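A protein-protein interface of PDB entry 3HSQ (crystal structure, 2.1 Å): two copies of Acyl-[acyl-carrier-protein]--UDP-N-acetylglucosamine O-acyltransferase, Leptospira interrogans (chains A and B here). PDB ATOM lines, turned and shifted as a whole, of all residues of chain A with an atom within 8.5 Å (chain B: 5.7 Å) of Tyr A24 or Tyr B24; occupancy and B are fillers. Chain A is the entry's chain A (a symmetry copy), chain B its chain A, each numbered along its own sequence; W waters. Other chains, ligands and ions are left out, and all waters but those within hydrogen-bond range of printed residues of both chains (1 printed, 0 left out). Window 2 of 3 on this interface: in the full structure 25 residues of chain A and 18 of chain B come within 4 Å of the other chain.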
ATOM      1  N   ILE A   3     -34.900   8.928  29.989  1.00  0.00           N
ATOM      2  CA  ILE A   3     -33.619   8.573  29.417  1.00  0.00           C
ATOM      3  C   ILE A   3     -33.906   7.906  28.074  1.00  0.00           C
ATOM      4  O   ILE A   3     -34.575   6.872  28.015  1.00  0.00           O
ATOM      5  CB  ILE A   3     -32.829   7.621  30.341  1.00  0.00           C
ATOM      6  CG1 ILE A   3     -32.433   8.341  31.638  1.00  0.00           C
ATOM      7  CG2 ILE A   3     -31.604   7.065  29.627  1.00  0.00           C
ATOM      8  CD1 ILE A   3     -32.115   7.422  32.806  1.00  0.00           C
ATOM      9  N   HIS A   4     -33.417   8.517  26.999  1.00  0.00           N
ATOM     10  CA  HIS A   4     -33.555   7.959  25.657  1.00  0.00           C
ATOM     11  C   HIS A   4     -32.963   6.548  25.600  1.00  0.00           C
ATOM     12  O   HIS A   4     -31.910   6.302  26.190  1.00  0.00           O
ATOM     13  CB  HIS A   4     -32.875   8.861  24.628  1.00  0.00           C
ATOM     14  CG  HIS A   4     -33.375   8.659  23.233  1.00  0.00           C
ATOM     15  ND1 HIS A   4     -32.741   7.840  22.325  1.00  0.00           N
ATOM     16  CD2 HIS A   4     -34.456   9.164  22.593  1.00  0.00           C
ATOM     17  CE1 HIS A   4     -33.407   7.850  21.185  1.00  0.00           C
ATOM     18  NE2 HIS A   4     -34.452   8.645  21.322  1.00  0.00           N
ATOM     19  N   PRO A   5     -33.655   5.612  24.911  1.00  0.00           N
ATOM     20  CA  PRO A   5     -33.226   4.210  24.795  1.00  0.00           C
ATOM     21  C   PRO A   5     -31.812   4.020  24.239  1.00  0.00           C
ATOM     22  O   PRO A   5     -31.179   2.995  24.516  1.00  0.00           O
ATOM     23  CB  PRO A   5     -34.253   3.614  23.827  1.00  0.00           C
ATOM     24  CG  PRO A   5     -35.462   4.453  24.012  1.00  0.00           C
ATOM     25  CD  PRO A   5     -34.940   5.840  24.220  1.00  0.00           C
ATOM     26  N   THR A   6     -31.326   5.004  23.481  1.00  0.00           N
ATOM     27  CA  THR A   6     -30.003   4.932  22.851  1.00  0.00           C
ATOM     28  C   THR A   6     -28.865   5.453  23.735  1.00  0.00           C
ATOM     29  O   THR A   6     -27.692   5.306  23.385  1.00  0.00           O
ATOM     30  CB  THR A   6     -29.966   5.680  21.499  1.00  0.00           C
ATOM     31  OG1 THR A   6     -30.173   7.085  21.715  1.00  0.00           O
ATOM     32  CG2 THR A   6     -31.031   5.143  20.547  1.00  0.00           C
ATOM     33  N   ALA A   7     -29.212   6.066  24.864  1.00  0.00           N
ATOM     34  CA  ALA A   7     -28.211   6.520  25.830  1.00  0.00           C
ATOM     35  C   ALA A   7     -27.495   5.328  26.461  1.00  0.00           C
ATOM     36  O   ALA A   7     -28.107   4.283  26.705  1.00  0.00           O
ATOM     37  CB  ALA A   7     -28.847   7.401  26.908  1.00  0.00           C
ATOM     38  N   ILE A   8     -26.199   5.485  26.704  1.00  0.00           N
ATOM     39  CA  ILE A   8     -25.403   4.425  27.299  1.00  0.00           C
ATOM     40  C   ILE A   8     -24.983   4.848  28.709  1.00  0.00           C
ATOM     41  O   ILE A   8     -24.005   5.585  28.894  1.00  0.00           O
ATOM     42  CB  ILE A   8     -24.199   4.028  26.393  1.00  0.00           C
ATOM     43  CG1 ILE A   8     -24.705   3.652  24.992  1.00  0.00           C
ATOM     44  CG2 ILE A   8     -23.410   2.876  27.009  1.00  0.00           C
ATOM     45  CD1 ILE A   8     -23.623   3.419  23.960  1.00  0.00           C
ATOM     46  N   ILE A   9     -25.755   4.382  29.691  1.00  0.00           N
ATOM     47  CA  ILE A   9     -25.575   4.756  31.095  1.00  0.00           C
ATOM     48  C   ILE A   9     -25.142   3.559  31.947  1.00  0.00           C
ATOM     49  O   ILE A   9     -25.923   2.625  32.187  1.00  0.00           O
ATOM     50  CB  ILE A   9     -26.856   5.407  31.697  1.00  0.00           C
ATOM     51  CG1 ILE A   9     -27.301   6.614  30.861  1.00  0.00           C
ATOM     52  CG2 ILE A   9     -26.631   5.800  33.160  1.00  0.00           C
ATOM     53  CD1 ILE A   9     -28.555   7.295  31.361  1.00  0.00           C
ATOM     54  N   VAL A  21     -31.795  12.406  30.106  1.00  0.00           N
ATOM     55  CA  VAL A  21     -30.618  12.108  29.295  1.00  0.00           C
ATOM     56  C   VAL A  21     -31.055  11.847  27.851  1.00  0.00           C
ATOM     57  O   VAL A  21     -31.856  10.939  27.590  1.00  0.00           O
ATOM     58  CB  VAL A  21     -29.820  10.891  29.845  1.00  0.00           C
ATOM     59  CG1 VAL A  21     -28.531  10.701  29.066  1.00  0.00           C
ATOM     60  CG2 VAL A  21     -29.511  11.060  31.331  1.00  0.00           C
ATOM     61  N   GLY A  22     -30.528  12.643  26.921  1.00  0.00           N
ATOM     62  CA  GLY A  22     -30.907  12.562  25.510  1.00  0.00           C
ATOM     63  C   GLY A  22     -30.159  11.530  24.681  1.00  0.00           C
ATOM     64  O   GLY A  22     -29.355  10.769  25.213  1.00  0.00           O
ATOM     65  N   PRO A  23     -30.409  11.514  23.359  1.00  0.00           N
ATOM     66  CA  PRO A  23     -29.944  10.467  22.456  1.00  0.00           C
ATOM     67  C   PRO A  23     -28.433  10.383  22.253  1.00  0.00           C
ATOM     68  O   PRO A  23     -27.766  11.398  21.988  1.00  0.00           O
ATOM     69  CB  PRO A  23     -30.630  10.817  21.127  1.00  0.00           C
ATOM     70  CG  PRO A  23     -31.693  11.800  21.461  1.00  0.00           C
ATOM     71  CD  PRO A  23     -31.198  12.535  22.644  1.00  0.00           C
ATOM     72  N   TYR A  24     -27.915   9.158  22.360  1.00  0.00           N
ATOM     73  CA  TYR A  24     -26.511   8.838  22.059  1.00  0.00           C
ATOM     74  C   TYR A  24     -25.533   9.451  23.068  1.00  0.00           C
ATOM     75  O   TYR A  24     -24.344   9.596  22.794  1.00  0.00           O
ATOM     76  CB  TYR A  24     -26.163   9.173  20.589  1.00  0.00           C
ATOM     77  CG  TYR A  24     -27.195   8.627  19.622  1.00  0.00           C
ATOM     78  CD1 TYR A  24     -28.034   9.472  18.902  1.00  0.00           C
ATOM     79  CD2 TYR A  24     -27.361   7.253  19.468  1.00  0.00           C
ATOM     80  CE1 TYR A  24     -29.003   8.954  18.029  1.00  0.00           C
ATOM     81  CE2 TYR A  24     -28.319   6.727  18.614  1.00  0.00           C
ATOM     82  CZ  TYR A  24     -29.139   7.577  17.898  1.00  0.00           C
ATOM     83  OH  TYR A  24     -30.080   7.022  17.052  1.00  0.00           O
ATOM     84  N   SER A  25     -26.049   9.780  24.246  1.00  0.00           N
ATOM     85  CA  SER A  25     -25.224  10.263  25.349  1.00  0.00           C
ATOM     86  C   SER A  25     -24.587   9.112  26.132  1.00  0.00           C
ATOM     87  O   SER A  25     -25.166   8.028  26.258  1.00  0.00           O
ATOM     88  CB  SER A  25     -26.042  11.161  26.277  1.00  0.00           C
ATOM     89  OG  SER A  25     -26.333  12.387  25.636  1.00  0.00           O
ATOM     90  N   ILE A  26     -23.387   9.358  26.645  1.00  0.00           N
ATOM     91  CA  ILE A  26     -22.623   8.355  27.361  1.00  0.00           C
ATOM     92  C   ILE A  26     -22.376   8.834  28.789  1.00  0.00           C
ATOM     93  O   ILE A  26     -21.823   9.916  29.010  1.00  0.00           O
ATOM     94  CB  ILE A  26     -21.282   8.038  26.628  1.00  0.00           C
ATOM     95  CG1 ILE A  26     -21.553   7.605  25.183  1.00  0.00           C
ATOM     96  CG2 ILE A  26     -20.487   6.961  27.360  1.00  0.00           C
ATOM     97  CD1 ILE A  26     -20.362   7.744  24.243  1.00  0.00           C
ATOM     98  N   ILE A  27     -22.823   8.044  29.760  1.00  0.00           N
ATOM     99  CA  ILE A  27     -22.516   8.318  31.166  1.00  0.00           C
ATOM    100  C   ILE A  27     -21.765   7.120  31.751  1.00  0.00           C
ATOM    101  O   ILE A  27     -22.233   5.967  31.672  1.00  0.00           O
ATOM    102  CB  ILE A  27     -23.770   8.652  32.020  1.00  0.00           C
ATOM    103  CG1 ILE A  27     -24.574   9.800  31.400  1.00  0.00           C
ATOM    104  CG2 ILE A  27     -23.357   9.034  33.421  1.00  0.00           C
ATOM    105  CD1 ILE A  27     -25.892  10.105  32.107  1.00  0.00           C
ATOM    106  N   ILE A  39     -29.491  16.431  30.414  1.00  0.00           N
ATOM    107  CA  ILE A  39     -28.412  16.147  29.481  1.00  0.00           C
ATOM    108  C   ILE A  39     -29.019  15.914  28.093  1.00  0.00           C
ATOM    109  O   ILE A  39     -29.866  15.032  27.922  1.00  0.00           O
ATOM    110  CB  ILE A  39     -27.609  14.909  29.932  1.00  0.00           C
ATOM    111  CG1 ILE A  39     -26.812  15.221  31.203  1.00  0.00           C
ATOM    112  CG2 ILE A  39     -26.685  14.426  28.814  1.00  0.00           C
ATOM    113  CD1 ILE A  39     -26.480  14.003  32.059  1.00  0.00           C
ATOM    114  N   GLU A  40     -28.593  16.710  27.116  1.00  0.00           N
ATOM    115  CA  GLU A  40     -29.067  16.583  25.738  1.00  0.00           C
ATOM    116  C   GLU A  40     -28.403  15.405  25.014  1.00  0.00           C
ATOM    117  O   GLU A  40     -28.023  14.413  25.646  1.00  0.00           O
ATOM    118  CB  GLU A  40     -28.869  17.900  24.970  1.00  0.00           C
ATOM    119  CG  GLU A  40     -29.840  19.017  25.358  1.00  0.00           C
ATOM    120  CD  GLU A  40     -29.565  20.348  24.653  1.00  0.00           C
ATOM    121  OE1 GLU A  40     -28.829  20.382  23.634  1.00  0.00           O
ATOM    122  OE2 GLU A  40     -30.101  21.377  25.127  1.00  0.00           O
ATOM    123  N   GLY A  41     -28.281  15.504  23.692  1.00  0.00           N
ATOM    124  CA  GLY A  41     -27.697  14.438  22.889  1.00  0.00           C
ATOM    125  C   GLY A  41     -26.183  14.459  22.814  1.00  0.00           C
ATOM    126  O   GLY A  41     -25.561  15.504  23.028  1.00  0.00           O
ATOM    127  N   HIS A  42     -25.594  13.294  22.537  1.00  0.00           N
ATOM    128  CA  HIS A  42     -24.134  13.147  22.291  1.00  0.00           C
ATOM    129  C   HIS A  42     -23.217  13.702  23.399  1.00  0.00           C
ATOM    130  O   HIS A  42     -22.017  13.931  23.179  1.00  0.00           O
ATOM    131  CB  HIS A  42     -23.754  13.768  20.936  1.00  0.00           C
ATOM    132  CG  HIS A  42     -24.547  13.232  19.787  1.00  0.00           C
ATOM    133  ND1 HIS A  42     -25.521  13.967  19.146  1.00  0.00           N
ATOM    134  CD2 HIS A  42     -24.522  12.024  19.174  1.00  0.00           C
ATOM    135  CE1 HIS A  42     -26.060  13.238  18.185  1.00  0.00           C
ATOM    136  NE2 HIS A  42     -25.471  12.054  18.181  1.00  0.00           N
ATOM    137  N   VAL A  43     -23.787  13.902  24.583  1.00  0.00           N
ATOM    138  CA  VAL A  43     -23.029  14.367  25.741  1.00  0.00           C
ATOM    139  C   VAL A  43     -22.256  13.192  26.348  1.00  0.00           C
ATOM    140  O   VAL A  43     -22.737  12.054  26.346  1.00  0.00           O
ATOM    141  CB  VAL A  43     -23.969  15.052  26.785  1.00  0.00           C
ATOM    142  CG1 VAL A  43     -23.255  15.343  28.097  1.00  0.00           C
ATOM    143  CG2 VAL A  43     -24.575  16.324  26.213  1.00  0.00           C
ATOM    144  N   LYS A  44     -21.044  13.460  26.824  1.00  0.00           N
ATOM    145  CA  LYS A  44     -20.304  12.463  27.586  1.00  0.00           C
ATOM    146  C   LYS A  44     -20.005  12.935  29.007  1.00  0.00           C
ATOM    147  O   LYS A  44     -19.418  14.001  29.214  1.00  0.00           O
ATOM    148  CB  LYS A  44     -19.002  12.076  26.886  1.00  0.00           C
ATOM    149  CG  LYS A  44     -18.340  10.839  27.469  1.00  0.00           C
ATOM    150  CD  LYS A  44     -16.863  10.831  27.128  1.00  0.00           C
ATOM    151  CE  LYS A  44     -16.349   9.425  26.971  1.00  0.00           C
ATOM    152  NZ  LYS A  44     -14.962   9.445  26.411  1.00  0.00           N
ATOM    153  N   GLN A  59     -25.856  19.555  23.603  1.00  0.00           N
ATOM    154  CA  GLN A  59     -25.291  18.583  22.673  1.00  0.00           C
ATOM    155  C   GLN A  59     -23.767  18.609  22.570  1.00  0.00           C
ATOM    156  O   GLN A  59     -23.175  19.658  22.309  1.00  0.00           O
ATOM    157  CB  GLN A  59     -25.922  18.751  21.281  1.00  0.00           C
ATOM    158  CG  GLN A  59     -25.211  17.954  20.180  1.00  0.00           C
ATOM    159  CD  GLN A  59     -26.145  17.271  19.200  1.00  0.00           C
ATOM    160  OE1 GLN A  59     -27.342  17.080  19.460  1.00  0.00           O
ATOM    161  NE2 GLN A  59     -25.597  16.890  18.059  1.00  0.00           N
ATOM    162  N   GLY A  60     -23.141  17.453  22.785  1.00  0.00           N
ATOM    163  CA  GLY A  60     -21.696  17.302  22.553  1.00  0.00           C
ATOM    164  C   GLY A  60     -20.776  17.822  23.649  1.00  0.00           C
ATOM    165  O   GLY A  60     -19.555  17.767  23.517  1.00  0.00           O
ATOM    166  N   HIS B   4     -17.739  -1.656  19.534  1.00  0.00           N
ATOM    167  CA  HIS B   4     -19.112  -1.474  19.997  1.00  0.00           C
ATOM    168  C   HIS B   4     -20.102  -1.767  18.866  1.00  0.00           C
ATOM    169  O   HIS B   4     -19.854  -1.383  17.721  1.00  0.00           O
ATOM    170  CB  HIS B   4     -19.316  -0.056  20.526  1.00  0.00           C
ATOM    171  CG  HIS B   4     -20.482   0.074  21.454  1.00  0.00           C
ATOM    172  ND1 HIS B   4     -21.726   0.493  21.034  1.00  0.00           N
ATOM    173  CD2 HIS B   4     -20.596  -0.172  22.781  1.00  0.00           C
ATOM    174  CE1 HIS B   4     -22.555   0.503  22.062  1.00  0.00           C
ATOM    175  NE2 HIS B   4     -21.895   0.104  23.133  1.00  0.00           N
ATOM    176  N   THR B   6     -22.767  -0.478  17.976  1.00  0.00           N
ATOM    177  CA  THR B   6     -23.332   0.721  17.348  1.00  0.00           C
ATOM    178  C   THR B   6     -22.363   1.447  16.409  1.00  0.00           C
ATOM    179  O   THR B   6     -22.761   2.376  15.703  1.00  0.00           O
ATOM    180  CB  THR B   6     -23.860   1.728  18.395  1.00  0.00           C
ATOM    181  OG1 THR B   6     -22.767   2.229  19.180  1.00  0.00           O
ATOM    182  CG2 THR B   6     -24.894   1.076  19.308  1.00  0.00           C
ATOM    183  N   ALA B   7     -21.098   1.032  16.412  1.00  0.00           N
ATOM    184  CA  ALA B   7     -20.105   1.588  15.491  1.00  0.00           C
ATOM    185  C   ALA B   7     -20.437   1.205  14.052  1.00  0.00           C
ATOM    186  O   ALA B   7     -20.921   0.100  13.788  1.00  0.00           O
ATOM    187  CB  ALA B   7     -18.694   1.127  15.861  1.00  0.00           C
ATOM    188  N   ILE B   8     -20.195   2.130  13.129  1.00  0.00           N
ATOM    189  CA  ILE B   8     -20.470   1.892  11.722  1.00  0.00           C
ATOM    190  C   ILE B   8     -19.145   1.815  10.960  1.00  0.00           C
ATOM    191  O   ILE B   8     -18.554   2.840  10.595  1.00  0.00           O
ATOM    192  CB  ILE B   8     -21.453   2.951  11.139  1.00  0.00           C
ATOM    193  CG1 ILE B   8     -22.739   2.985  11.980  1.00  0.00           C
ATOM    194  CG2 ILE B   8     -21.773   2.650   9.677  1.00  0.00           C
ATOM    195  CD1 ILE B   8     -23.705   4.097  11.630  1.00  0.00           C
ATOM    196  N   GLY B  22     -15.183   2.676  19.809  1.00  0.00           N
ATOM    197  CA  GLY B  22     -16.285   2.965  20.725  1.00  0.00           C
ATOM    198  C   GLY B  22     -17.612   3.320  20.074  1.00  0.00           C
ATOM    199  O   GLY B  22     -17.738   3.274  18.853  1.00  0.00           O
ATOM    200  N   PRO B  23     -18.610   3.699  20.895  1.00  0.00           N
ATOM    201  CA  PRO B  23     -19.993   3.871  20.466  1.00  0.00           C
ATOM    202  C   PRO B  23     -20.252   5.018  19.489  1.00  0.00           C
ATOM    203  O   PRO B  23     -19.807   6.157  19.709  1.00  0.00           O
ATOM    204  CB  PRO B  23     -20.741   4.130  21.782  1.00  0.00           C
ATOM    205  CG  PRO B  23     -19.808   3.731  22.868  1.00  0.00           C
ATOM    206  CD  PRO B  23     -18.451   3.973  22.333  1.00  0.00           C
ATOM    207  N   TYR B  24     -20.993   4.699  18.428  1.00  0.00           N
ATOM    208  CA  TYR B  24     -21.477   5.683  17.446  1.00  0.00           C
ATOM    209  C   TYR B  24     -20.348   6.288  16.605  1.00  0.00           C
ATOM    210  O   TYR B  24     -20.498   7.351  16.007  1.00  0.00           O
ATOM    211  CB  TYR B  24     -22.375   6.749  18.119  1.00  0.00           C
ATOM    212  CG  TYR B  24     -23.429   6.124  19.014  1.00  0.00           C
ATOM    213  CD1 TYR B  24     -23.387   6.269  20.396  1.00  0.00           C
ATOM    214  CD2 TYR B  24     -24.442   5.339  18.469  1.00  0.00           C
ATOM    215  CE1 TYR B  24     -24.352   5.663  21.215  1.00  0.00           C
ATOM    216  CE2 TYR B  24     -25.399   4.729  19.266  1.00  0.00           C
ATOM    217  CZ  TYR B  24     -25.351   4.890  20.637  1.00  0.00           C
ATOM    218  OH  TYR B  24     -26.322   4.274  21.403  1.00  0.00           O
ATOM    219  N   SER B  25     -19.227   5.578  16.548  1.00  0.00           N
ATOM    220  CA  SER B  25     -18.106   5.961  15.694  1.00  0.00           C
ATOM    221  C   SER B  25     -18.295   5.478  14.253  1.00  0.00           C
ATOM    222  O   SER B  25     -18.893   4.426  14.006  1.00  0.00           O
ATOM    223  CB  SER B  25     -16.791   5.441  16.272  1.00  0.00           C
ATOM    224  OG  SER B  25     -16.458   6.155  17.445  1.00  0.00           O
ATOM    225  N   ILE B  26     -17.786   6.263  13.311  1.00  0.00           N
ATOM    226  CA  ILE B  26     -17.932   5.979  11.896  1.00  0.00           C
ATOM    227  C   ILE B  26     -16.550   5.798  11.274  1.00  0.00           C
ATOM    228  O   ILE B  26     -15.692   6.681  11.365  1.00  0.00           O
ATOM    229  CB  ILE B  26     -18.738   7.106  11.176  1.00  0.00           C
ATOM    230  CG1 ILE B  26     -20.102   7.301  11.848  1.00  0.00           C
ATOM    231  CG2 ILE B  26     -18.920   6.798   9.692  1.00  0.00           C
ATOM    232  CD1 ILE B  26     -20.757   8.650  11.576  1.00  0.00           C
ATOM    233  N   GLY B  41     -15.808   7.226  21.410  1.00  0.00           N
ATOM    234  CA  GLY B  41     -17.132   7.432  20.841  1.00  0.00           C
ATOM    235  C   GLY B  41     -17.226   8.581  19.856  1.00  0.00           C
ATOM    236  O   GLY B  41     -16.398   9.496  19.883  1.00  0.00           O
ATOM    237  N   HIS B  42     -18.219   8.511  18.968  1.00  0.00           N
ATOM    238  CA  HIS B  42     -18.549   9.605  18.014  1.00  0.00           C
ATOM    239  C   HIS B  42     -17.381  10.092  17.134  1.00  0.00           C
ATOM    240  O   HIS B  42     -17.436  11.184  16.547  1.00  0.00           O
ATOM    241  CB  HIS B  42     -19.174  10.797  18.761  1.00  0.00           C
ATOM    242  CG  HIS B  42     -20.365  10.428  19.587  1.00  0.00           C
ATOM    243  ND1 HIS B  42     -20.332  10.384  20.965  1.00  0.00           N
ATOM    244  CD2 HIS B  42     -21.621  10.069  19.229  1.00  0.00           C
ATOM    245  CE1 HIS B  42     -21.517  10.017  21.420  1.00  0.00           C
ATOM    246  NE2 HIS B  42     -22.318   9.821  20.386  1.00  0.00           N
ATOM    247  N   VAL B  43     -16.340   9.272  17.041  1.00  0.00           N
ATOM    248  CA  VAL B  43     -15.187   9.572  16.197  1.00  0.00           C
ATOM    249  C   VAL B  43     -15.529   9.251  14.738  1.00  0.00           C
ATOM    250  O   VAL B  43     -16.261   8.297  14.458  1.00  0.00           O
ATOM    251  CB  VAL B  43     -13.919   8.799  16.685  1.00  0.00           C
ATOM    252  CG1 VAL B  43     -12.765   8.909  15.701  1.00  0.00           C
ATOM    253  CG2 VAL B  43     -13.494   9.279  18.065  1.00  0.00           C
HETATM  254  O   HOH W   1     -16.107   8.606  23.793  1.00  0.00           O
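Among the printed residues, merely in contact across the chains: Ile A8 with His B4 (3.6 Å), Ile A8 with Pro B23 (3.7 Å), Ile A8 with Tyr B24 (3.6 Å), Tyr A24 with Tyr B24 (3.2 Å), Ile A26 with His B42 (3.8 Å) and His A42 with His B42 (3.3 Å).
Tyr A24 touches two residues of chain B. Of the printed residues of chain B, Ile A26 touches His B42 (3.8 Å). Of the printed residues of chain A, His B4 touches Ile A8. Ile A9 touches none of the printed residues of chain B. The nearest printed residue of chain B that does not touch Tyr A24 is Pro B23 (6.5 Å). The nearest residue of chain A that does not touch Tyr B24 is Ala A7 (4.9 Å).
O of Tyr A24 lies within hydrogen-bond range of NE2 of His B42, at 3.2 Å. OH of Tyr B24 lies within hydrogen-bond range of O of Thr A6, at 2.6 Å.
Water W1 lies within hydrogen-bond range of N of Gly B41 (2.8 Å) and NZ of Lys A44 (3.0 Å).
Of the 12 printed residues of chain B, 4 touch a printed residue of chain A. Hydrophobic or aromatic side chains of chain B that line the printed part of chain A: His B4, Pro B23, Tyr B24 and His B42. Among the printed residues, 8 pairs touch across the chains.
Ile A8 touches His B4, but with the chains exchanged His A4 does not touch Ile B8 (14.1 Å). Ile A8 touches Tyr B24, but with the chains exchanged Tyr A24 does not touch Ile B8 (8.8 Å). Tyr A24 touches His B42, but with the chains exchanged His A42 does not touch Tyr B24 (5.8 Å). His A42 touches its own counterpart, His B42. 12 positions are printed for both chains.
The side-chain hydroxyl (OG1) of Thr B6 lies within hydrogen-bond range of the backbone NH (N) of Tyr B24 (3.1 Å). N of Ile A27 lies within hydrogen-bond range of O of Ile A8, at 2.9 Å. The side-chain hydroxyl (OG1) of Thr A6 lies within hydrogen-bond range of the backbone NH (N) of Tyr A24, at 3.1 Å. N of His B42 sits at hydrogen-bond distance from OG of Ser B25 (3.3 Å). O of Pro B23 lies within hydrogen-bond range of N of His B42, 2.9 Å away. The side-chain hydroxyl (OG) of Ser A25 sits at hydrogen-bond distance from the backbone NH (N) of His A42, at 3.3 Å.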
